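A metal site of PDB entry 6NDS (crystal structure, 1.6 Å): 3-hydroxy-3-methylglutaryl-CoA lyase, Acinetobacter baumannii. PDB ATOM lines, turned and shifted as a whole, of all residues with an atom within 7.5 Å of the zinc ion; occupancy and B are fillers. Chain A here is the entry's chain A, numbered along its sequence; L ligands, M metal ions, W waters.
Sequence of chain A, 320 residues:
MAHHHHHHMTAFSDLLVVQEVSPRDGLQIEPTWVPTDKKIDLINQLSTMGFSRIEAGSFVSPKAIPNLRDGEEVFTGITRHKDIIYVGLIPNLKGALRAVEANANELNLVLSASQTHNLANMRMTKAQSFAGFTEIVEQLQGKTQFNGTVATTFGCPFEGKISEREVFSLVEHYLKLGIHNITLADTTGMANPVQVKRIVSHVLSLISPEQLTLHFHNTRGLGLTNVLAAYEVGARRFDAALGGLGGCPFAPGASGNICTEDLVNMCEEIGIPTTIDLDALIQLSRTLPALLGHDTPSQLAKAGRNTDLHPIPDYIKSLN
Merely in contact with the zinc ion: Asn 257. Of the 22 residues printed, 4 come within 4 Å of the zinc ion. The nearest printed residue that does not touch the zinc ion is Arg 24 (4.1 Å).
OD2 of Asp 25 binds the zinc ion, 2.1 Å away. The zinc ion is bound by O1 of LIG L1 (2.1 Å). The zinc ion is bound by O5 of LIG L1, at 2.2 Å. NE2 of His 215 is bound to the zinc ion (2.2 Å). The zinc ion is bound by a ring nitrogen (NE2) of His 217, at 2.2 Å. The zinc ion is bound by water W1 (2.2 Å). The zinc ion has six donor atoms within binding distance.
N of His 217 sits close to O of Asp 186. ND1 of His 217 lies within hydrogen-bond range of O of Ser 255 (2.8 Å). The side-chain carboxylate of Asp 25 sits close to the side-chain amide nitrogen of Asn 257, 3.0 Å away. NE2 of His 215 lies close to ND2 of Asn 257, 3.3 Å away. OD1 of Asp 25 sits at hydrogen-bond distance from N of Gly 247 (3.3 Å). The backbone NH (N) of Asn 257 is in hydrogen-bond range of a ring nitrogen (ND1) of His 217. A ring nitrogen (ND1) of His 215 is in hydrogen-bond range of the side-chain carboxylate of Asp 239, 2.9 Å away. A ring nitrogen (ND1) of His 217 is in hydrogen-bond range of the backbone carbonyl oxygen of Gly 256 (3.4 Å).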
ATOM      1  N   VAL A  21     -20.411   6.336 -24.279  1.00  0.00           N
ATOM      2  CA  VAL A  21     -19.153   5.682 -23.887  1.00  0.00           C
ATOM      3  C   VAL A  21     -18.577   4.768 -24.972  1.00  0.00           C
ATOM      4  O   VAL A  21     -17.626   4.022 -24.715  1.00  0.00           O
ATOM      5  CB  VAL A  21     -19.312   4.888 -22.568  1.00  0.00           C
ATOM      6  CG1 VAL A  21     -19.817   5.804 -21.427  1.00  0.00           C
ATOM      7  CG2 VAL A  21     -20.240   3.676 -22.747  1.00  0.00           C
ATOM      8  N   ARG A  24     -14.692   4.472 -25.528  1.00  0.00           N
ATOM      9  CA  ARG A  24     -13.916   3.828 -24.472  1.00  0.00           C
ATOM     10  C   ARG A  24     -14.424   2.405 -24.247  1.00  0.00           C
ATOM     11  O   ARG A  24     -13.741   1.445 -24.630  1.00  0.00           O
ATOM     12  CB  ARG A  24     -13.993   4.674 -23.197  1.00  0.00           C
ATOM     13  CG  ARG A  24     -12.969   4.338 -22.093  1.00  0.00           C
ATOM     14  CD  ARG A  24     -13.323   3.055 -21.329  1.00  0.00           C
ATOM     15  NE  ARG A  24     -14.577   3.169 -20.591  1.00  0.00           N
ATOM     16  CZ  ARG A  24     -15.148   2.159 -19.934  1.00  0.00           C
ATOM     17  NH1 ARG A  24     -14.576   0.964 -19.939  1.00  0.00           N
ATOM     18  NH2 ARG A  24     -16.281   2.357 -19.273  1.00  0.00           N
ATOM     19  N   ASP A  25     -15.612   2.242 -23.666  1.00  0.00           N
ATOM     20  CA  ASP A  25     -16.127   0.894 -23.401  1.00  0.00           C
ATOM     21  C   ASP A  25     -16.332   0.137 -24.703  1.00  0.00           C
ATOM     22  O   ASP A  25     -16.052  -1.060 -24.783  1.00  0.00           O
ATOM     23  CB  ASP A  25     -17.433   1.002 -22.621  1.00  0.00           C
ATOM     24  CG  ASP A  25     -17.639  -0.152 -21.662  1.00  0.00           C
ATOM     25  OD1 ASP A  25     -17.075  -1.257 -21.881  1.00  0.00           O
ATOM     26  OD2 ASP A  25     -18.384   0.040 -20.687  1.00  0.00           O
ATOM     27  N   GLY A  26     -16.795   0.845 -25.733  1.00  0.00           N
ATOM     28  CA  GLY A  26     -17.066   0.188 -27.006  1.00  0.00           C
ATOM     29  C   GLY A  26     -15.817  -0.350 -27.662  1.00  0.00           C
ATOM     30  O   GLY A  26     -15.778  -1.481 -28.129  1.00  0.00           O
ATOM     31  N   GLN A  28     -12.633  -0.751 -26.354  1.00  0.00           N
ATOM     32  CA  GLN A  28     -11.584  -1.430 -25.612  1.00  0.00           C
ATOM     33  C   GLN A  28     -11.572  -2.933 -25.874  1.00  0.00           C
ATOM     34  O   GLN A  28     -10.512  -3.570 -25.827  1.00  0.00           O
ATOM     35  CB  GLN A  28     -11.722  -1.148 -24.113  1.00  0.00           C
ATOM     36  CG  GLN A  28     -12.953  -1.724 -23.505  1.00  0.00           C
ATOM     37  CD  GLN A  28     -13.143  -1.318 -22.057  1.00  0.00           C
ATOM     38  OE1 GLN A  28     -12.504  -0.384 -21.550  1.00  0.00           O
ATOM     39  NE2 GLN A  28     -14.040  -2.029 -21.373  1.00  0.00           N
ATOM     40  N   GLU A  55     -17.239   9.769 -23.043  1.00  0.00           N
ATOM     41  CA  GLU A  55     -16.019   9.165 -22.502  1.00  0.00           C
ATOM     42  C   GLU A  55     -15.150   8.843 -23.711  1.00  0.00           C
ATOM     43  O   GLU A  55     -15.398   7.873 -24.437  1.00  0.00           O
ATOM     44  CB  GLU A  55     -16.350   7.938 -21.663  1.00  0.00           C
ATOM     45  CG  GLU A  55     -15.191   7.529 -20.735  1.00  0.00           C
ATOM     46  CD  GLU A  55     -15.642   6.589 -19.628  1.00  0.00           C
ATOM     47  OE1 GLU A  55     -15.961   5.422 -19.937  1.00  0.00           O
ATOM     48  OE2 GLU A  55     -15.675   7.016 -18.451  1.00  0.00           O
ATOM     49  N   LEU A  89     -11.174   7.597 -18.577  1.00  0.00           N
ATOM     50  CA  LEU A  89     -11.167   6.568 -17.537  1.00  0.00           C
ATOM     51  C   LEU A  89      -9.757   6.399 -16.977  1.00  0.00           C
ATOM     52  O   LEU A  89      -8.784   6.284 -17.734  1.00  0.00           O
ATOM     53  CB  LEU A  89     -11.664   5.228 -18.090  1.00  0.00           C
ATOM     54  CG  LEU A  89     -11.701   4.061 -17.088  1.00  0.00           C
ATOM     55  CD1 LEU A  89     -12.852   3.130 -17.423  1.00  0.00           C
ATOM     56  CD2 LEU A  89     -10.404   3.253 -17.102  1.00  0.00           C
ATOM     57  N   ALA A 151     -17.581  -0.537 -10.094  1.00  0.00           N
ATOM     58  CA  ALA A 151     -17.886  -1.639 -11.001  1.00  0.00           C
ATOM     59  C   ALA A 151     -18.383  -2.861 -10.208  1.00  0.00           C
ATOM     60  O   ALA A 151     -18.287  -2.920  -8.983  1.00  0.00           O
ATOM     61  CB  ALA A 151     -16.667  -2.003 -11.846  1.00  0.00           C
ATOM     62  N   ALA A 185     -21.957   0.651 -11.895  1.00  0.00           N
ATOM     63  CA  ALA A 185     -21.829  -0.082 -13.153  1.00  0.00           C
ATOM     64  C   ALA A 185     -22.196  -1.551 -12.977  1.00  0.00           C
ATOM     65  O   ALA A 185     -21.703  -2.212 -12.058  1.00  0.00           O
ATOM     66  CB  ALA A 185     -20.399   0.053 -13.702  1.00  0.00           C
ATOM     67  N   ASP A 186     -23.037  -2.051 -13.895  1.00  0.00           N
ATOM     68  CA  ASP A 186     -23.376  -3.477 -14.007  1.00  0.00           C
ATOM     69  C   ASP A 186     -22.502  -4.097 -15.096  1.00  0.00           C
ATOM     70  O   ASP A 186     -22.904  -4.297 -16.244  1.00  0.00           O
ATOM     71  CB  ASP A 186     -24.863  -3.639 -14.337  1.00  0.00           C
ATOM     72  CG  ASP A 186     -25.295  -5.071 -14.383  1.00  0.00           C
ATOM     73  OD1 ASP A 186     -24.545  -5.926 -13.871  1.00  0.00           O
ATOM     74  OD2 ASP A 186     -26.373  -5.349 -14.933  1.00  0.00           O
ATOM     75  N   THR A 187     -21.271  -4.449 -14.686  1.00  0.00           N
ATOM     76  CA  THR A 187     -20.200  -4.772 -15.613  1.00  0.00           C
ATOM     77  C   THR A 187     -20.513  -5.953 -16.521  1.00  0.00           C
ATOM     78  O   THR A 187     -20.161  -5.947 -17.703  1.00  0.00           O
ATOM     79  CB  THR A 187     -18.928  -5.037 -14.804  1.00  0.00           C
ATOM     80  OG1 THR A 187     -18.728  -3.935 -13.923  1.00  0.00           O
ATOM     81  CG2 THR A 187     -17.720  -5.202 -15.730  1.00  0.00           C
ATOM     82  N   THR A 188     -21.124  -7.016 -15.987  1.00  0.00           N
ATOM     83  CA  THR A 188     -21.465  -8.156 -16.831  1.00  0.00           C
ATOM     84  C   THR A 188     -22.971  -8.409 -16.889  1.00  0.00           C
ATOM     85  O   THR A 188     -23.399  -9.543 -17.086  1.00  0.00           O
ATOM     86  CB  THR A 188     -20.742  -9.431 -16.385  1.00  0.00           C
ATOM     87  OG1 THR A 188     -21.130  -9.756 -15.054  1.00  0.00           O
ATOM     88  CG2 THR A 188     -19.235  -9.231 -16.474  1.00  0.00           C
ATOM     89  N   HIS A 215     -24.685   2.663 -15.241  1.00  0.00           N
ATOM     90  CA  HIS A 215     -23.947   2.138 -16.393  1.00  0.00           C
ATOM     91  C   HIS A 215     -24.297   0.663 -16.546  1.00  0.00           C
ATOM     92  O   HIS A 215     -23.697  -0.201 -15.903  1.00  0.00           O
ATOM     93  CB  HIS A 215     -22.467   2.379 -16.132  1.00  0.00           C
ATOM     94  CG  HIS A 215     -21.530   1.837 -17.174  1.00  0.00           C
ATOM     95  ND1 HIS A 215     -20.767   2.647 -17.980  1.00  0.00           N
ATOM     96  CD2 HIS A 215     -21.156   0.558 -17.458  1.00  0.00           C
ATOM     97  CE1 HIS A 215     -19.999   1.905 -18.750  1.00  0.00           C
ATOM     98  NE2 HIS A 215     -20.222   0.627 -18.467  1.00  0.00           N
ATOM     99  N   PHE A 216     -25.298   0.347 -17.378  1.00  0.00           N
ATOM    100  CA  PHE A 216     -25.777  -1.022 -17.535  1.00  0.00           C
ATOM    101  C   PHE A 216     -25.212  -1.684 -18.788  1.00  0.00           C
ATOM    102  O   PHE A 216     -25.149  -1.069 -19.859  1.00  0.00           O
ATOM    103  CB  PHE A 216     -27.314  -1.068 -17.594  1.00  0.00           C
ATOM    104  CG  PHE A 216     -27.990  -0.671 -16.313  1.00  0.00           C
ATOM    105  CD1 PHE A 216     -27.888  -1.470 -15.177  1.00  0.00           C
ATOM    106  CD2 PHE A 216     -28.783   0.463 -16.254  1.00  0.00           C
ATOM    107  CE1 PHE A 216     -28.536  -1.108 -13.981  1.00  0.00           C
ATOM    108  CE2 PHE A 216     -29.455   0.820 -15.075  1.00  0.00           C
ATOM    109  CZ  PHE A 216     -29.316   0.025 -13.941  1.00  0.00           C
ATOM    110  N   HIS A 217     -24.810  -2.936 -18.671  1.00  0.00           N
ATOM    111  CA  HIS A 217     -24.567  -3.757 -19.837  1.00  0.00           C
ATOM    112  C   HIS A 217     -25.777  -4.667 -20.073  1.00  0.00           C
ATOM    113  O   HIS A 217     -26.586  -4.898 -19.162  1.00  0.00           O
ATOM    114  CB  HIS A 217     -23.261  -4.560 -19.669  1.00  0.00           C
ATOM    115  CG  HIS A 217     -22.010  -3.721 -19.775  1.00  0.00           C
ATOM    116  ND1 HIS A 217     -21.221  -3.718 -20.912  1.00  0.00           N
ATOM    117  CD2 HIS A 217     -21.422  -2.868 -18.900  1.00  0.00           C
ATOM    118  CE1 HIS A 217     -20.194  -2.897 -20.723  1.00  0.00           C
ATOM    119  NE2 HIS A 217     -20.305  -2.363 -19.519  1.00  0.00           N
ATOM    120  N   ASP A 239     -25.202   5.862 -18.929  1.00  0.00           N
ATOM    121  CA  ASP A 239     -24.201   5.589 -19.950  1.00  0.00           C
ATOM    122  C   ASP A 239     -24.751   4.617 -21.005  1.00  0.00           C
ATOM    123  O   ASP A 239     -25.474   3.671 -20.684  1.00  0.00           O
ATOM    124  CB  ASP A 239     -22.945   4.970 -19.332  1.00  0.00           C
ATOM    125  CG  ASP A 239     -22.122   5.950 -18.497  1.00  0.00           C
ATOM    126  OD1 ASP A 239     -22.321   7.186 -18.601  1.00  0.00           O
ATOM    127  OD2 ASP A 239     -21.245   5.467 -17.745  1.00  0.00           O
ATOM    128  N   GLY A 246     -19.325  -2.766 -26.830  1.00  0.00           N
ATOM    129  CA  GLY A 246     -18.730  -2.667 -25.501  1.00  0.00           C
ATOM    130  C   GLY A 246     -18.519  -3.999 -24.811  1.00  0.00           C
ATOM    131  O   GLY A 246     -18.834  -5.065 -25.320  1.00  0.00           O
ATOM    132  N   GLY A 247     -17.953  -3.906 -23.601  1.00  0.00           N
ATOM    133  CA  GLY A 247     -17.586  -5.047 -22.783  1.00  0.00           C
ATOM    134  C   GLY A 247     -16.182  -4.852 -22.252  1.00  0.00           C
ATOM    135  O   GLY A 247     -15.356  -4.154 -22.846  1.00  0.00           O
ATOM    136  N   CYS A 248     -15.889  -5.479 -21.088  1.00  0.00           N
ATOM    137  CA  CYS A 248     -14.550  -5.428 -20.509  1.00  0.00           C
ATOM    138  C   CYS A 248     -13.802  -6.718 -20.813  1.00  0.00           C
ATOM    139  O   CYS A 248     -14.351  -7.810 -20.578  1.00  0.00           O
ATOM    140  CB  CYS A 248     -14.608  -5.205 -19.001  1.00  0.00           C
ATOM    141  SG  CYS A 248     -12.998  -5.338 -18.133  1.00  0.00           S
ATOM    142  N   SER A 255     -20.185  -8.261 -22.389  1.00  0.00           N
ATOM    143  CA  SER A 255     -20.783  -7.977 -23.686  1.00  0.00           C
ATOM    144  C   SER A 255     -21.206  -6.507 -23.695  1.00  0.00           C
ATOM    145  O   SER A 255     -20.825  -5.718 -22.821  1.00  0.00           O
ATOM    146  CB  SER A 255     -21.939  -8.944 -23.966  1.00  0.00           C
ATOM    147  OG  SER A 255     -23.063  -8.631 -23.174  1.00  0.00           O
ATOM    148  N   GLY A 256     -22.019  -6.142 -24.685  1.00  0.00           N
ATOM    149  CA  GLY A 256     -22.181  -4.743 -25.019  1.00  0.00           C
ATOM    150  C   GLY A 256     -22.877  -3.936 -23.941  1.00  0.00           C
ATOM    151  O   GLY A 256     -23.692  -4.422 -23.159  1.00  0.00           O
ATOM    152  N   ASN A 257     -22.521  -2.662 -23.898  1.00  0.00           N
ATOM    153  CA  ASN A 257     -23.308  -1.673 -23.192  1.00  0.00           C
ATOM    154  C   ASN A 257     -24.718  -1.643 -23.764  1.00  0.00           C
ATOM    155  O   ASN A 257     -24.973  -2.100 -24.888  1.00  0.00           O
ATOM    156  CB  ASN A 257     -22.695  -0.290 -23.360  1.00  0.00           C
ATOM    157  CG  ASN A 257     -21.332  -0.185 -22.742  1.00  0.00           C
ATOM    158  OD1 ASN A 257     -20.325  -0.609 -23.330  1.00  0.00           O
ATOM    159  ND2 ASN A 257     -21.275   0.391 -21.545  1.00  0.00           N
HETATM  160  C1  LIG L   1     -17.371   1.137 -15.907  1.00  0.00           C
HETATM  161  C2  LIG L   1     -16.988  -0.151 -16.613  1.00  0.00           C
HETATM  162  O1  LIG L   1     -17.110   0.052 -17.988  1.00  0.00           O
HETATM  163  C3  LIG L   1     -15.528  -0.508 -16.392  1.00  0.00           C
HETATM  164  C4  LIG L   1     -15.064  -1.699 -17.156  1.00  0.00           C
HETATM  165  O2  LIG L   1     -14.779  -2.799 -16.555  1.00  0.00           O
HETATM  166  O3  LIG L   1     -14.907  -1.670 -18.418  1.00  0.00           O
HETATM  167  C5  LIG L   1     -17.847  -1.302 -16.139  1.00  0.00           C
HETATM  168  O4  LIG L   1     -17.659  -1.847 -15.026  1.00  0.00           O
HETATM  169  O5  LIG L   1     -18.781  -1.756 -16.881  1.00  0.00           O
HETATM  170  N1  LG2 L   2      -1.122   4.090 -17.967  1.00  0.00           N
HETATM  171  C1  LG2 L   2      -0.032   3.657 -18.621  1.00  0.00           C
HETATM  172  N2  LG2 L   2       1.021   2.989 -18.158  1.00  0.00           N
HETATM  173  C2  LG2 L   2       0.887   2.738 -16.844  1.00  0.00           C
HETATM  174  C3  LG2 L   2      -0.184   3.099 -16.036  1.00  0.00           C
HETATM  175  C4  LG2 L   2      -1.235   3.812 -16.640  1.00  0.00           C
HETATM  176  N3  LG2 L   2      -2.311   4.228 -15.985  1.00  0.00           N
HETATM  177  N4  LG2 L   2       0.036   2.677 -14.737  1.00  0.00           N
HETATM  178  C5  LG2 L   2       1.209   2.068 -14.774  1.00  0.00           C
HETATM  179  N5  LG2 L   2       1.757   2.074 -16.026  1.00  0.00           N
HETATM  180  C6  LG2 L   2       3.061   1.521 -16.433  1.00  0.00           C
HETATM  181  C7  LG2 L   2       4.249   2.072 -15.660  1.00  0.00           C
HETATM  182  O1  LG2 L   2       4.693   3.338 -16.066  1.00  0.00           O
HETATM  183  C8  LG2 L   2       5.255   0.945 -15.888  1.00  0.00           C
HETATM  184  O2  LG2 L   2       5.708   0.949 -17.235  1.00  0.00           O
HETATM  185  P1  LG2 L   2       7.090   0.123 -17.369  1.00  0.00           P
HETATM  186  O3  LG2 L   2       6.740  -1.353 -17.521  1.00  0.00           O
HETATM  187  O4  LG2 L   2       7.859   0.396 -16.096  1.00  0.00           O
HETATM  188  O5  LG2 L   2       7.797   0.669 -18.586  1.00  0.00           O
HETATM  189  C9  LG2 L   2       4.343  -0.238 -15.597  1.00  0.00           C
HETATM  190  O6  LG2 L   2       3.072   0.128 -16.224  1.00  0.00           O
HETATM  191  C10 LG2 L   2       4.100  -0.392 -14.117  1.00  0.00           C
HETATM  192  O7  LG2 L   2       3.264  -1.543 -13.892  1.00  0.00           O
HETATM  193  P2  LG2 L   2       2.503  -1.606 -12.492  1.00  0.00           P
HETATM  194  O8  LG2 L   2       2.437  -0.259 -11.871  1.00  0.00           O
HETATM  195  O9  LG2 L   2       3.013  -2.766 -11.697  1.00  0.00           O
HETATM  196  O10 LG2 L   2       1.038  -1.947 -13.050  1.00  0.00           O
HETATM  197  P3  LG2 L   2       0.426  -3.276 -13.691  1.00  0.00           P
HETATM  198  O11 LG2 L   2       0.196  -4.272 -12.602  1.00  0.00           O
HETATM  199  O12 LG2 L   2       1.217  -3.685 -14.884  1.00  0.00           O
HETATM  200  O13 LG2 L   2      -0.976  -2.689 -14.210  1.00  0.00           O
HETATM  201  C11 LG2 L   2      -2.824  -1.176 -14.109  1.00  0.00           C
HETATM  202  C12 LG2 L   2      -1.860  -2.026 -13.282  1.00  0.00           C
HETATM  203  C13 LG2 L   2      -3.913  -0.579 -13.220  1.00  0.00           C
HETATM  204  C14 LG2 L   2      -2.044  -0.033 -14.770  1.00  0.00           C
HETATM  205  C15 LG2 L   2      -3.430  -2.091 -15.173  1.00  0.00           C
HETATM  206  O14 LG2 L   2      -3.963  -3.245 -14.545  1.00  0.00           O
HETATM  207  C16 LG2 L   2      -4.542  -1.419 -15.980  1.00  0.00           C
HETATM  208  O15 LG2 L   2      -4.278  -0.549 -16.794  1.00  0.00           O
HETATM  209  N6  LG2 L   2      -5.772  -1.846 -15.741  1.00  0.00           N
HETATM  210  C17 LG2 L   2      -6.952  -1.235 -16.342  1.00  0.00           C
HETATM  211  C18 LG2 L   2      -7.601  -2.148 -17.343  1.00  0.00           C
HETATM  212  C19 LG2 L   2      -8.920  -1.587 -17.850  1.00  0.00           C
HETATM  213  O16 LG2 L   2      -8.991  -0.431 -18.261  1.00  0.00           O
HETATM  214  N7  LG2 L   2      -9.969  -2.410 -17.827  1.00  0.00           N
HETATM  215  C20 LG2 L   2     -11.254  -2.110 -18.430  1.00  0.00           C
HETATM  216  C21 LG2 L   2     -11.886  -0.861 -17.852  1.00  0.00           C
HETATM  217  S1  LG2 L   2     -11.996  -0.942 -16.049  1.00  0.00           S
HETATM  218 ZN    ZN M   1     -18.759  -0.931 -18.890  1.00  0.00          ZN
HETATM  219  O   HOH W   1     -17.210  -2.405 -19.448  1.00  0.00           O
